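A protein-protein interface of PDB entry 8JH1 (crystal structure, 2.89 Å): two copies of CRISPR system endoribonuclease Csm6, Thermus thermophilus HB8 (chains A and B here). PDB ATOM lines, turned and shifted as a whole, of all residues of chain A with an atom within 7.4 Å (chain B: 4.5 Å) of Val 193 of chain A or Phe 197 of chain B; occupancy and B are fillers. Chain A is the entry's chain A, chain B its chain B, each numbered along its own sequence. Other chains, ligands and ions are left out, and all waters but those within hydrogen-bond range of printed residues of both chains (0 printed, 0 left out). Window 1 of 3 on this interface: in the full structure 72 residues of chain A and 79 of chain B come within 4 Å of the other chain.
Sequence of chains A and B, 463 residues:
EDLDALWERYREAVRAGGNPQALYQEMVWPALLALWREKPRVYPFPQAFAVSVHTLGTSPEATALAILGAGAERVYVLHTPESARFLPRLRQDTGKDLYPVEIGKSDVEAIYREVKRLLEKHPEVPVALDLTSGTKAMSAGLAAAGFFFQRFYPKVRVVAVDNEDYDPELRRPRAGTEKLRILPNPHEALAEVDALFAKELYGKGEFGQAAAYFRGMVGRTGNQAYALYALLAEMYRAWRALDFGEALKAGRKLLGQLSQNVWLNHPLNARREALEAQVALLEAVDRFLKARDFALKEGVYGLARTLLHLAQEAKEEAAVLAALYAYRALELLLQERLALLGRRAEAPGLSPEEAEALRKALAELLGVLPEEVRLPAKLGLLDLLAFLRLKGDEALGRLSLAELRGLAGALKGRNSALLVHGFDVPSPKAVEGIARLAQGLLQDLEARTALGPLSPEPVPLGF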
ATOM      1  N   PHE A 148      29.386 -22.166  -1.747  1.00  0.00           N
ATOM      2  CA  PHE A 148      28.607 -21.380  -2.694  1.00  0.00           C
ATOM      3  C   PHE A 148      27.214 -21.071  -2.150  1.00  0.00           C
ATOM      4  O   PHE A 148      26.799 -19.910  -2.106  1.00  0.00           O
ATOM      5  CB  PHE A 148      28.526 -22.096  -4.041  1.00  0.00           C
ATOM      6  CG  PHE A 148      27.653 -21.399  -5.023  1.00  0.00           C
ATOM      7  CD1 PHE A 148      28.153 -20.371  -5.802  1.00  0.00           C
ATOM      8  CD2 PHE A 148      26.327 -21.751  -5.157  1.00  0.00           C
ATOM      9  CE1 PHE A 148      27.345 -19.707  -6.704  1.00  0.00           C
ATOM     10  CE2 PHE A 148      25.516 -21.091  -6.046  1.00  0.00           C
ATOM     11  CZ  PHE A 148      26.027 -20.057  -6.824  1.00  0.00           C
ATOM     12  N   ARG A 151      25.914 -18.294   0.757  1.00  0.00           N
ATOM     13  CA  ARG A 151      25.470 -16.920   0.567  1.00  0.00           C
ATOM     14  C   ARG A 151      23.959 -16.830   0.607  1.00  0.00           C
ATOM     15  O   ARG A 151      23.390 -15.966   1.282  1.00  0.00           O
ATOM     16  CB  ARG A 151      25.980 -16.397  -0.764  1.00  0.00           C
ATOM     17  CG  ARG A 151      25.345 -15.120  -1.206  1.00  0.00           C
ATOM     18  CD  ARG A 151      25.951 -14.717  -2.522  1.00  0.00           C
ATOM     19  NE  ARG A 151      25.924 -13.276  -2.710  1.00  0.00           N
ATOM     20  CZ  ARG A 151      26.813 -12.442  -2.194  1.00  0.00           C
ATOM     21  NH1 ARG A 151      27.829 -12.879  -1.465  1.00  0.00           N
ATOM     22  NH2 ARG A 151      26.701 -11.139  -2.436  1.00  0.00           N
ATOM     23  N   PHE A 152      23.291 -17.747  -0.089  1.00  0.00           N
ATOM     24  CA  PHE A 152      21.847 -17.745  -0.221  1.00  0.00           C
ATOM     25  C   PHE A 152      21.146 -18.591   0.831  1.00  0.00           C
ATOM     26  O   PHE A 152      19.920 -18.501   0.950  1.00  0.00           O
ATOM     27  CB  PHE A 152      21.469 -18.248  -1.604  1.00  0.00           C
ATOM     28  CG  PHE A 152      22.344 -17.725  -2.704  1.00  0.00           C
ATOM     29  CD1 PHE A 152      22.261 -16.403  -3.113  1.00  0.00           C
ATOM     30  CD2 PHE A 152      23.240 -18.564  -3.344  1.00  0.00           C
ATOM     31  CE1 PHE A 152      23.051 -15.929  -4.145  1.00  0.00           C
ATOM     32  CE2 PHE A 152      24.029 -18.107  -4.378  1.00  0.00           C
ATOM     33  CZ  PHE A 152      23.933 -16.785  -4.781  1.00  0.00           C
ATOM     34  N   HIS A 187      34.983 -18.045   0.460  1.00  0.00           N
ATOM     35  CA  HIS A 187      34.261 -17.086  -0.375  1.00  0.00           C
ATOM     36  C   HIS A 187      33.716 -15.955   0.477  1.00  0.00           C
ATOM     37  O   HIS A 187      33.998 -14.776   0.223  1.00  0.00           O
ATOM     38  CB  HIS A 187      33.093 -17.743  -1.114  1.00  0.00           C
ATOM     39  CG  HIS A 187      33.502 -18.764  -2.125  1.00  0.00           C
ATOM     40  ND1 HIS A 187      34.785 -18.852  -2.628  1.00  0.00           N
ATOM     41  CD2 HIS A 187      32.777 -19.711  -2.772  1.00  0.00           C
ATOM     42  CE1 HIS A 187      34.843 -19.837  -3.508  1.00  0.00           C
ATOM     43  NE2 HIS A 187      33.636 -20.369  -3.621  1.00  0.00           N
ATOM     44  N   GLU A 188      32.946 -16.315   1.513  1.00  0.00           N
ATOM     45  CA  GLU A 188      32.448 -15.347   2.482  1.00  0.00           C
ATOM     46  C   GLU A 188      33.587 -14.511   3.071  1.00  0.00           C
ATOM     47  O   GLU A 188      33.599 -13.274   2.968  1.00  0.00           O
ATOM     48  CB  GLU A 188      31.733 -16.077   3.612  1.00  0.00           C
ATOM     49  CG  GLU A 188      30.235 -16.204   3.596  1.00  0.00           C
ATOM     50  CD  GLU A 188      29.698 -16.065   5.036  1.00  0.00           C
ATOM     51  OE1 GLU A 188      29.693 -14.920   5.563  1.00  0.00           O
ATOM     52  OE2 GLU A 188      29.384 -17.105   5.680  1.00  0.00           O
ATOM     53  N   LEU A 190      36.510 -13.760   2.399  1.00  0.00           N
ATOM     54  CA  LEU A 190      37.158 -12.803   1.528  1.00  0.00           C
ATOM     55  C   LEU A 190      36.148 -11.907   0.837  1.00  0.00           C
ATOM     56  O   LEU A 190      36.529 -10.863   0.294  1.00  0.00           O
ATOM     57  CB  LEU A 190      38.017 -13.547   0.507  1.00  0.00           C
ATOM     58  CG  LEU A 190      39.317 -14.191   0.989  1.00  0.00           C
ATOM     59  CD1 LEU A 190      39.125 -15.259   2.083  1.00  0.00           C
ATOM     60  CD2 LEU A 190      39.989 -14.811  -0.219  1.00  0.00           C
ATOM     61  N   ALA A 191      34.871 -12.297   0.876  1.00  0.00           N
ATOM     62  CA  ALA A 191      33.784 -11.554   0.248  1.00  0.00           C
ATOM     63  C   ALA A 191      34.090 -11.284  -1.217  1.00  0.00           C
ATOM     64  O   ALA A 191      33.895 -10.171  -1.710  1.00  0.00           O
ATOM     65  CB  ALA A 191      33.508 -10.251   0.997  1.00  0.00           C
ATOM     66  N   GLU A 192      34.603 -12.308  -1.914  1.00  0.00           N
ATOM     67  CA  GLU A 192      34.959 -12.124  -3.319  1.00  0.00           C
ATOM     68  C   GLU A 192      33.733 -11.761  -4.141  1.00  0.00           C
ATOM     69  O   GLU A 192      33.820 -10.966  -5.084  1.00  0.00           O
ATOM     70  CB  GLU A 192      35.623 -13.377  -3.895  1.00  0.00           C
ATOM     71  CG  GLU A 192      36.710 -14.032  -3.054  1.00  0.00           C
ATOM     72  CD  GLU A 192      37.956 -14.391  -3.881  1.00  0.00           C
ATOM     73  OE1 GLU A 192      38.687 -13.495  -4.376  1.00  0.00           O
ATOM     74  OE2 GLU A 192      38.193 -15.594  -4.068  1.00  0.00           O
ATOM     75  N   VAL A 193      32.577 -12.333  -3.800  1.00  0.00           N
ATOM     76  CA  VAL A 193      31.374 -12.050  -4.569  1.00  0.00           C
ATOM     77  C   VAL A 193      30.884 -10.635  -4.295  1.00  0.00           C
ATOM     78  O   VAL A 193      30.518  -9.906  -5.229  1.00  0.00           O
ATOM     79  CB  VAL A 193      30.287 -13.093  -4.270  1.00  0.00           C
ATOM     80  CG1 VAL A 193      28.919 -12.538  -4.610  1.00  0.00           C
ATOM     81  CG2 VAL A 193      30.561 -14.350  -5.051  1.00  0.00           C
ATOM     82  N   ASP A 194      30.822 -10.238  -3.012  1.00  0.00           N
ATOM     83  CA  ASP A 194      30.422  -8.871  -2.691  1.00  0.00           C
ATOM     84  C   ASP A 194      31.321  -7.886  -3.406  1.00  0.00           C
ATOM     85  O   ASP A 194      30.853  -6.880  -3.937  1.00  0.00           O
ATOM     86  CB  ASP A 194      30.471  -8.626  -1.188  1.00  0.00           C
ATOM     87  CG  ASP A 194      29.352  -9.307  -0.456  1.00  0.00           C
ATOM     88  OD1 ASP A 194      28.850 -10.323  -0.987  1.00  0.00           O
ATOM     89  OD2 ASP A 194      28.978  -8.835   0.648  1.00  0.00           O
ATOM     90  N   ALA A 195      32.613  -8.186  -3.464  1.00  0.00           N
ATOM     91  CA  ALA A 195      33.515  -7.372  -4.266  1.00  0.00           C
ATOM     92  C   ALA A 195      33.094  -7.358  -5.730  1.00  0.00           C
ATOM     93  O   ALA A 195      33.050  -6.296  -6.349  1.00  0.00           O
ATOM     94  CB  ALA A 195      34.953  -7.881  -4.138  1.00  0.00           C
ATOM     95  N   LEU A 196      32.813  -8.532  -6.316  1.00  0.00           N
ATOM     96  CA  LEU A 196      32.519  -8.573  -7.749  1.00  0.00           C
ATOM     97  C   LEU A 196      31.288  -7.733  -8.066  1.00  0.00           C
ATOM     98  O   LEU A 196      31.280  -6.950  -9.030  1.00  0.00           O
ATOM     99  CB  LEU A 196      32.357 -10.028  -8.220  1.00  0.00           C
ATOM    100  CG  LEU A 196      33.550 -10.568  -9.031  1.00  0.00           C
ATOM    101  CD1 LEU A 196      33.587  -9.924 -10.417  1.00  0.00           C
ATOM    102  CD2 LEU A 196      34.868 -10.294  -8.324  1.00  0.00           C
ATOM    103  N   PHE A 197      30.265  -7.839  -7.221  1.00  0.00           N
ATOM    104  CA  PHE A 197      29.073  -7.018  -7.384  1.00  0.00           C
ATOM    105  C   PHE A 197      29.398  -5.548  -7.209  1.00  0.00           C
ATOM    106  O   PHE A 197      28.999  -4.718  -8.031  1.00  0.00           O
ATOM    107  CB  PHE A 197      27.983  -7.452  -6.407  1.00  0.00           C
ATOM    108  CG  PHE A 197      27.178  -8.642  -6.893  1.00  0.00           C
ATOM    109  CD1 PHE A 197      26.411  -9.402  -6.019  1.00  0.00           C
ATOM    110  CD2 PHE A 197      27.212  -9.009  -8.234  1.00  0.00           C
ATOM    111  CE1 PHE A 197      25.689 -10.467  -6.469  1.00  0.00           C
ATOM    112  CE2 PHE A 197      26.495 -10.086  -8.694  1.00  0.00           C
ATOM    113  CZ  PHE A 197      25.730 -10.816  -7.805  1.00  0.00           C
ATOM    114  N   ALA A 198      30.131  -5.206  -6.149  1.00  0.00           N
ATOM    115  CA  ALA A 198      30.473  -3.808  -5.912  1.00  0.00           C
ATOM    116  C   ALA A 198      31.288  -3.241  -7.062  1.00  0.00           C
ATOM    117  O   ALA A 198      31.125  -2.075  -7.431  1.00  0.00           O
ATOM    118  CB  ALA A 198      31.227  -3.654  -4.594  1.00  0.00           C
ATOM    119  N   LYS A 199      32.157  -4.059  -7.648  1.00  0.00           N
ATOM    120  CA  LYS A 199      32.915  -3.641  -8.819  1.00  0.00           C
ATOM    121  C   LYS A 199      31.991  -3.395  -9.997  1.00  0.00           C
ATOM    122  O   LYS A 199      32.150  -2.410 -10.729  1.00  0.00           O
ATOM    123  CB  LYS A 199      33.949  -4.706  -9.161  1.00  0.00           C
ATOM    124  CG  LYS A 199      34.657  -4.470 -10.462  1.00  0.00           C
ATOM    125  CD  LYS A 199      36.137  -4.432 -10.199  1.00  0.00           C
ATOM    126  CE  LYS A 199      36.909  -3.976 -11.414  1.00  0.00           C
ATOM    127  NZ  LYS A 199      37.868  -5.049 -11.798  1.00  0.00           N
ATOM    128  N   TYR A 213      27.532  -2.451  -0.591  1.00  0.00           N
ATOM    129  CA  TYR A 213      28.215  -3.734  -0.678  1.00  0.00           C
ATOM    130  C   TYR A 213      29.544  -3.702   0.044  1.00  0.00           C
ATOM    131  O   TYR A 213      29.912  -4.664   0.724  1.00  0.00           O
ATOM    132  CB  TYR A 213      28.434  -4.124  -2.125  1.00  0.00           C
ATOM    133  CG  TYR A 213      27.357  -5.036  -2.596  1.00  0.00           C
ATOM    134  CD1 TYR A 213      27.372  -6.380  -2.259  1.00  0.00           C
ATOM    135  CD2 TYR A 213      26.309  -4.543  -3.358  1.00  0.00           C
ATOM    136  CE1 TYR A 213      26.373  -7.206  -2.683  1.00  0.00           C
ATOM    137  CE2 TYR A 213      25.315  -5.353  -3.788  1.00  0.00           C
ATOM    138  CZ  TYR A 213      25.346  -6.682  -3.457  1.00  0.00           C
ATOM    139  OH  TYR A 213      24.328  -7.488  -3.900  1.00  0.00           O
ATOM    140  N   MET A 217      30.858  -5.653   3.157  1.00  0.00           N
ATOM    141  CA  MET A 217      32.117  -6.349   2.993  1.00  0.00           C
ATOM    142  C   MET A 217      32.987  -6.222   4.233  1.00  0.00           C
ATOM    143  O   MET A 217      33.663  -7.178   4.631  1.00  0.00           O
ATOM    144  CB  MET A 217      32.817  -5.803   1.762  1.00  0.00           C
ATOM    145  CG  MET A 217      33.512  -6.834   0.990  1.00  0.00           C
ATOM    146  SD  MET A 217      33.800  -6.256  -0.678  1.00  0.00           S
ATOM    147  CE  MET A 217      35.308  -7.190  -0.966  1.00  0.00           C
ATOM    148  N   PHE B 148      35.645 -22.082  -7.896  1.00  0.00           N
ATOM    149  CA  PHE B 148      35.231 -20.695  -8.027  1.00  0.00           C
ATOM    150  C   PHE B 148      36.015 -19.944  -9.101  1.00  0.00           C
ATOM    151  O   PHE B 148      35.490 -18.998  -9.688  1.00  0.00           O
ATOM    152  CB  PHE B 148      35.367 -19.983  -6.692  1.00  0.00           C
ATOM    153  CG  PHE B 148      35.107 -18.521  -6.782  1.00  0.00           C
ATOM    154  CD1 PHE B 148      33.828 -18.057  -7.026  1.00  0.00           C
ATOM    155  CD2 PHE B 148      36.142 -17.604  -6.650  1.00  0.00           C
ATOM    156  CE1 PHE B 148      33.576 -16.711  -7.123  1.00  0.00           C
ATOM    157  CE2 PHE B 148      35.905 -16.243  -6.738  1.00  0.00           C
ATOM    158  CZ  PHE B 148      34.617 -15.794  -6.978  1.00  0.00           C
ATOM    159  N   ASP B 194      23.099 -19.849 -10.811  1.00  0.00           N
ATOM    160  CA  ASP B 194      23.503 -18.452 -10.910  1.00  0.00           C
ATOM    161  C   ASP B 194      22.301 -17.511 -10.879  1.00  0.00           C
ATOM    162  O   ASP B 194      22.481 -16.311 -10.624  1.00  0.00           O
ATOM    163  CB  ASP B 194      24.328 -18.205 -12.178  1.00  0.00           C
ATOM    164  CG  ASP B 194      25.756 -18.755 -12.079  1.00  0.00           C
ATOM    165  OD1 ASP B 194      26.391 -18.722 -10.992  1.00  0.00           O
ATOM    166  OD2 ASP B 194      26.251 -19.206 -13.133  1.00  0.00           O
ATOM    167  N   ALA B 195      21.083 -18.047 -11.086  1.00  0.00           N
ATOM    168  CA  ALA B 195      19.858 -17.258 -10.956  1.00  0.00           C
ATOM    169  C   ALA B 195      19.807 -16.504  -9.638  1.00  0.00           C
ATOM    170  O   ALA B 195      19.331 -15.360  -9.593  1.00  0.00           O
ATOM    171  CB  ALA B 195      18.637 -18.158 -11.078  1.00  0.00           C
ATOM    172  N   LEU B 196      20.300 -17.117  -8.549  1.00  0.00           N
ATOM    173  CA  LEU B 196      20.210 -16.445  -7.255  1.00  0.00           C
ATOM    174  C   LEU B 196      20.919 -15.090  -7.276  1.00  0.00           C
ATOM    175  O   LEU B 196      20.426 -14.125  -6.670  1.00  0.00           O
ATOM    176  CB  LEU B 196      20.759 -17.360  -6.167  1.00  0.00           C
ATOM    177  CG  LEU B 196      19.998 -18.697  -6.191  1.00  0.00           C
ATOM    178  CD1 LEU B 196      20.899 -19.918  -5.934  1.00  0.00           C
ATOM    179  CD2 LEU B 196      18.741 -18.703  -5.290  1.00  0.00           C
ATOM    180  N   PHE B 197      22.042 -14.992  -8.000  1.00  0.00           N
ATOM    181  CA  PHE B 197      22.721 -13.706  -8.169  1.00  0.00           C
ATOM    182  C   PHE B 197      21.822 -12.720  -8.898  1.00  0.00           C
ATOM    183  O   PHE B 197      21.652 -11.570  -8.464  1.00  0.00           O
ATOM    184  CB  PHE B 197      24.036 -13.893  -8.930  1.00  0.00           C
ATOM    185  CG  PHE B 197      25.073 -14.659  -8.170  1.00  0.00           C
ATOM    186  CD1 PHE B 197      25.357 -14.352  -6.852  1.00  0.00           C
ATOM    187  CD2 PHE B 197      25.754 -15.702  -8.770  1.00  0.00           C
ATOM    188  CE1 PHE B 197      26.319 -15.052  -6.154  1.00  0.00           C
ATOM    189  CE2 PHE B 197      26.713 -16.410  -8.074  1.00  0.00           C
ATOM    190  CZ  PHE B 197      26.996 -16.080  -6.762  1.00  0.00           C
ATOM    191  N   ALA B 198      21.205 -13.172  -9.997  1.00  0.00           N
ATOM    192  CA  ALA B 198      20.168 -12.370 -10.626  1.00  0.00           C
ATOM    193  C   ALA B 198      19.041 -12.079  -9.639  1.00  0.00           C
ATOM    194  O   ALA B 198      18.639 -10.916  -9.484  1.00  0.00           O
ATOM    195  CB  ALA B 198      19.653 -13.069 -11.879  1.00  0.00           C
ATOM    196  N   LYS B 199      18.597 -13.098  -8.877  1.00  0.00           N
ATOM    197  CA  LYS B 199      17.539 -12.846  -7.901  1.00  0.00           C
ATOM    198  C   LYS B 199      17.971 -11.766  -6.925  1.00  0.00           C
ATOM    199  O   LYS B 199      17.164 -10.918  -6.525  1.00  0.00           O
ATOM    200  CB  LYS B 199      17.150 -14.119  -7.137  1.00  0.00           C
ATOM    201  CG  LYS B 199      16.246 -13.819  -5.903  1.00  0.00           C
ATOM    202  CD  LYS B 199      16.015 -15.023  -4.982  1.00  0.00           C
ATOM    203  CE  LYS B 199      14.694 -14.898  -4.207  1.00  0.00           C
ATOM    204  NZ  LYS B 199      14.777 -14.337  -2.818  1.00  0.00           N
ATOM    205  N   GLU B 200      19.257 -11.766  -6.559  1.00  0.00           N
ATOM    206  CA  GLU B 200      19.754 -10.774  -5.619  1.00  0.00           C
ATOM    207  C   GLU B 200      19.854  -9.410  -6.284  1.00  0.00           C
ATOM    208  O   GLU B 200      19.436  -8.399  -5.706  1.00  0.00           O
ATOM    209  CB  GLU B 200      21.102 -11.234  -5.085  1.00  0.00           C
ATOM    210  CG  GLU B 200      21.735 -10.394  -3.991  1.00  0.00           C
ATOM    211  CD  GLU B 200      23.184 -10.792  -3.790  1.00  0.00           C
ATOM    212  OE1 GLU B 200      23.436 -11.986  -3.506  1.00  0.00           O
ATOM    213  OE2 GLU B 200      24.065  -9.925  -3.931  1.00  0.00           O
ATOM    214  N   LEU B 201      20.373  -9.371  -7.517  1.00  0.00           N
ATOM    215  CA  LEU B 201      20.489  -8.100  -8.226  1.00  0.00           C
ATOM    216  C   LEU B 201      19.108  -7.486  -8.421  1.00  0.00           C
ATOM    217  O   LEU B 201      18.934  -6.262  -8.330  1.00  0.00           O
ATOM    218  CB  LEU B 201      21.205  -8.312  -9.569  1.00  0.00           C
ATOM    219  CG  LEU B 201      22.723  -8.083  -9.707  1.00  0.00           C
ATOM    220  CD1 LEU B 201      23.247  -8.503 -11.075  1.00  0.00           C
ATOM    221  CD2 LEU B 201      23.102  -6.630  -9.465  1.00  0.00           C
ATOM    222  N   TYR B 213      21.910 -10.016 -16.413  1.00  0.00           N
ATOM    223  CA  TYR B 213      22.246 -11.305 -15.819  1.00  0.00           C
ATOM    224  C   TYR B 213      21.355 -12.402 -16.362  1.00  0.00           C
ATOM    225  O   TYR B 213      21.827 -13.478 -16.746  1.00  0.00           O
ATOM    226  CB  TYR B 213      22.120 -11.244 -14.300  1.00  0.00           C
ATOM    227  CG  TYR B 213      23.021 -12.236 -13.653  1.00  0.00           C
ATOM    228  CD1 TYR B 213      22.726 -13.582 -13.664  1.00  0.00           C
ATOM    229  CD2 TYR B 213      24.221 -11.834 -13.123  1.00  0.00           C
ATOM    230  CE1 TYR B 213      23.585 -14.499 -13.097  1.00  0.00           C
ATOM    231  CE2 TYR B 213      25.080 -12.724 -12.558  1.00  0.00           C
ATOM    232  CZ  TYR B 213      24.766 -14.060 -12.547  1.00  0.00           C
ATOM    233  OH  TYR B 213      25.651 -14.942 -11.973  1.00  0.00           O
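Phe 148 of chain A touches Phe 197 of chain B, but with the chains exchanged Phe 197 of chain A does not touch Phe 148 of chain B (9.1 Å). Phe 197 of chain A touches its own counterpart, Phe 197 of chain B. Positions printed for both chains: 148, 194, 195, 196, 197, 198, 199 and 213.
Of the 17 printed residues of chain A, 8 touch a printed residue of chain B. Of the 10 printed residues of chain B, 4 touch a printed residue of chain A. Among the printed residues, 11 pairs touch across the chains. Among the printed residues, Asp or Glu carboxylates within 4 Å of a Lys or Arg side-chain nitrogen of the other chain: Arg 151 of chain A with Glu 200 of chain B (2.9 Å).
The side-chain hydroxyl of Tyr 213 of chain A lies within hydrogen-bond range of the side-chain carboxylate of Glu 200 of chain B (2.5 Å). The guanidinium group of Arg 151 of chain A is in salt-bridge range of the side-chain carboxylate of Glu 200 of chain B (2.9 Å).
The guanidinium group (NH2) of Arg 151 of chain A lies within salt-bridge range of the side-chain carboxylate (OD1) of Asp 194 of chain A, 2.7 Å away. The backbone NH (N) of Glu 192 of chain A lies within hydrogen-bond range of the backbone carbonyl oxygen (O) of His 187 of chain A (3.3 Å).
Of the printed residues of chain B, Phe 148 of chain A touches Phe 197. Of the printed residues of chain B, Arg 151 of chain A touches Phe 197 and Glu 200. Of the printed residues of chain B, Phe 152 of chain A touches Leu 196 and Phe 197. Of the printed residues of chain B, His 187 of chain A touches Phe 148. Of chain B, only Phe 197 (3.9 Å) comes within 4 Å of Val 193 of chain A. Leu 196 of chain A touches none of the printed residues of chain B. Of the printed residues of chain A, Leu 196 of chain B touches Phe 152 (3.4 Å). Phe 197 of chain B touches five residues of chain A. The nearest residue of chain A that does not touch Phe 197 of chain B is Tyr 213 of chain A (6.7 Å). The nearest printed residue of chain B that does not touch Arg 151 of chain A is Leu 196 of chain B (6.8 Å).
Among the printed residues, pairs that only touch across the chains: Phe 148 of chain A with Phe 197 of chain B, Arg 151 of chain A with Phe 197 of chain B, Phe 152 of chain A with Leu 196 of chain B, Phe 152 of chain A with Phe 197 of chain B, His 187 of chain A with Phe 148 of chain B, Glu 192 of chain A with Phe 148 of chain B, Val 193 of chain A with Phe 197 of chain B, Phe 197 of chain A with Phe 197 of chain B and Phe 197 of chain A with Glu 200 of chain B.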
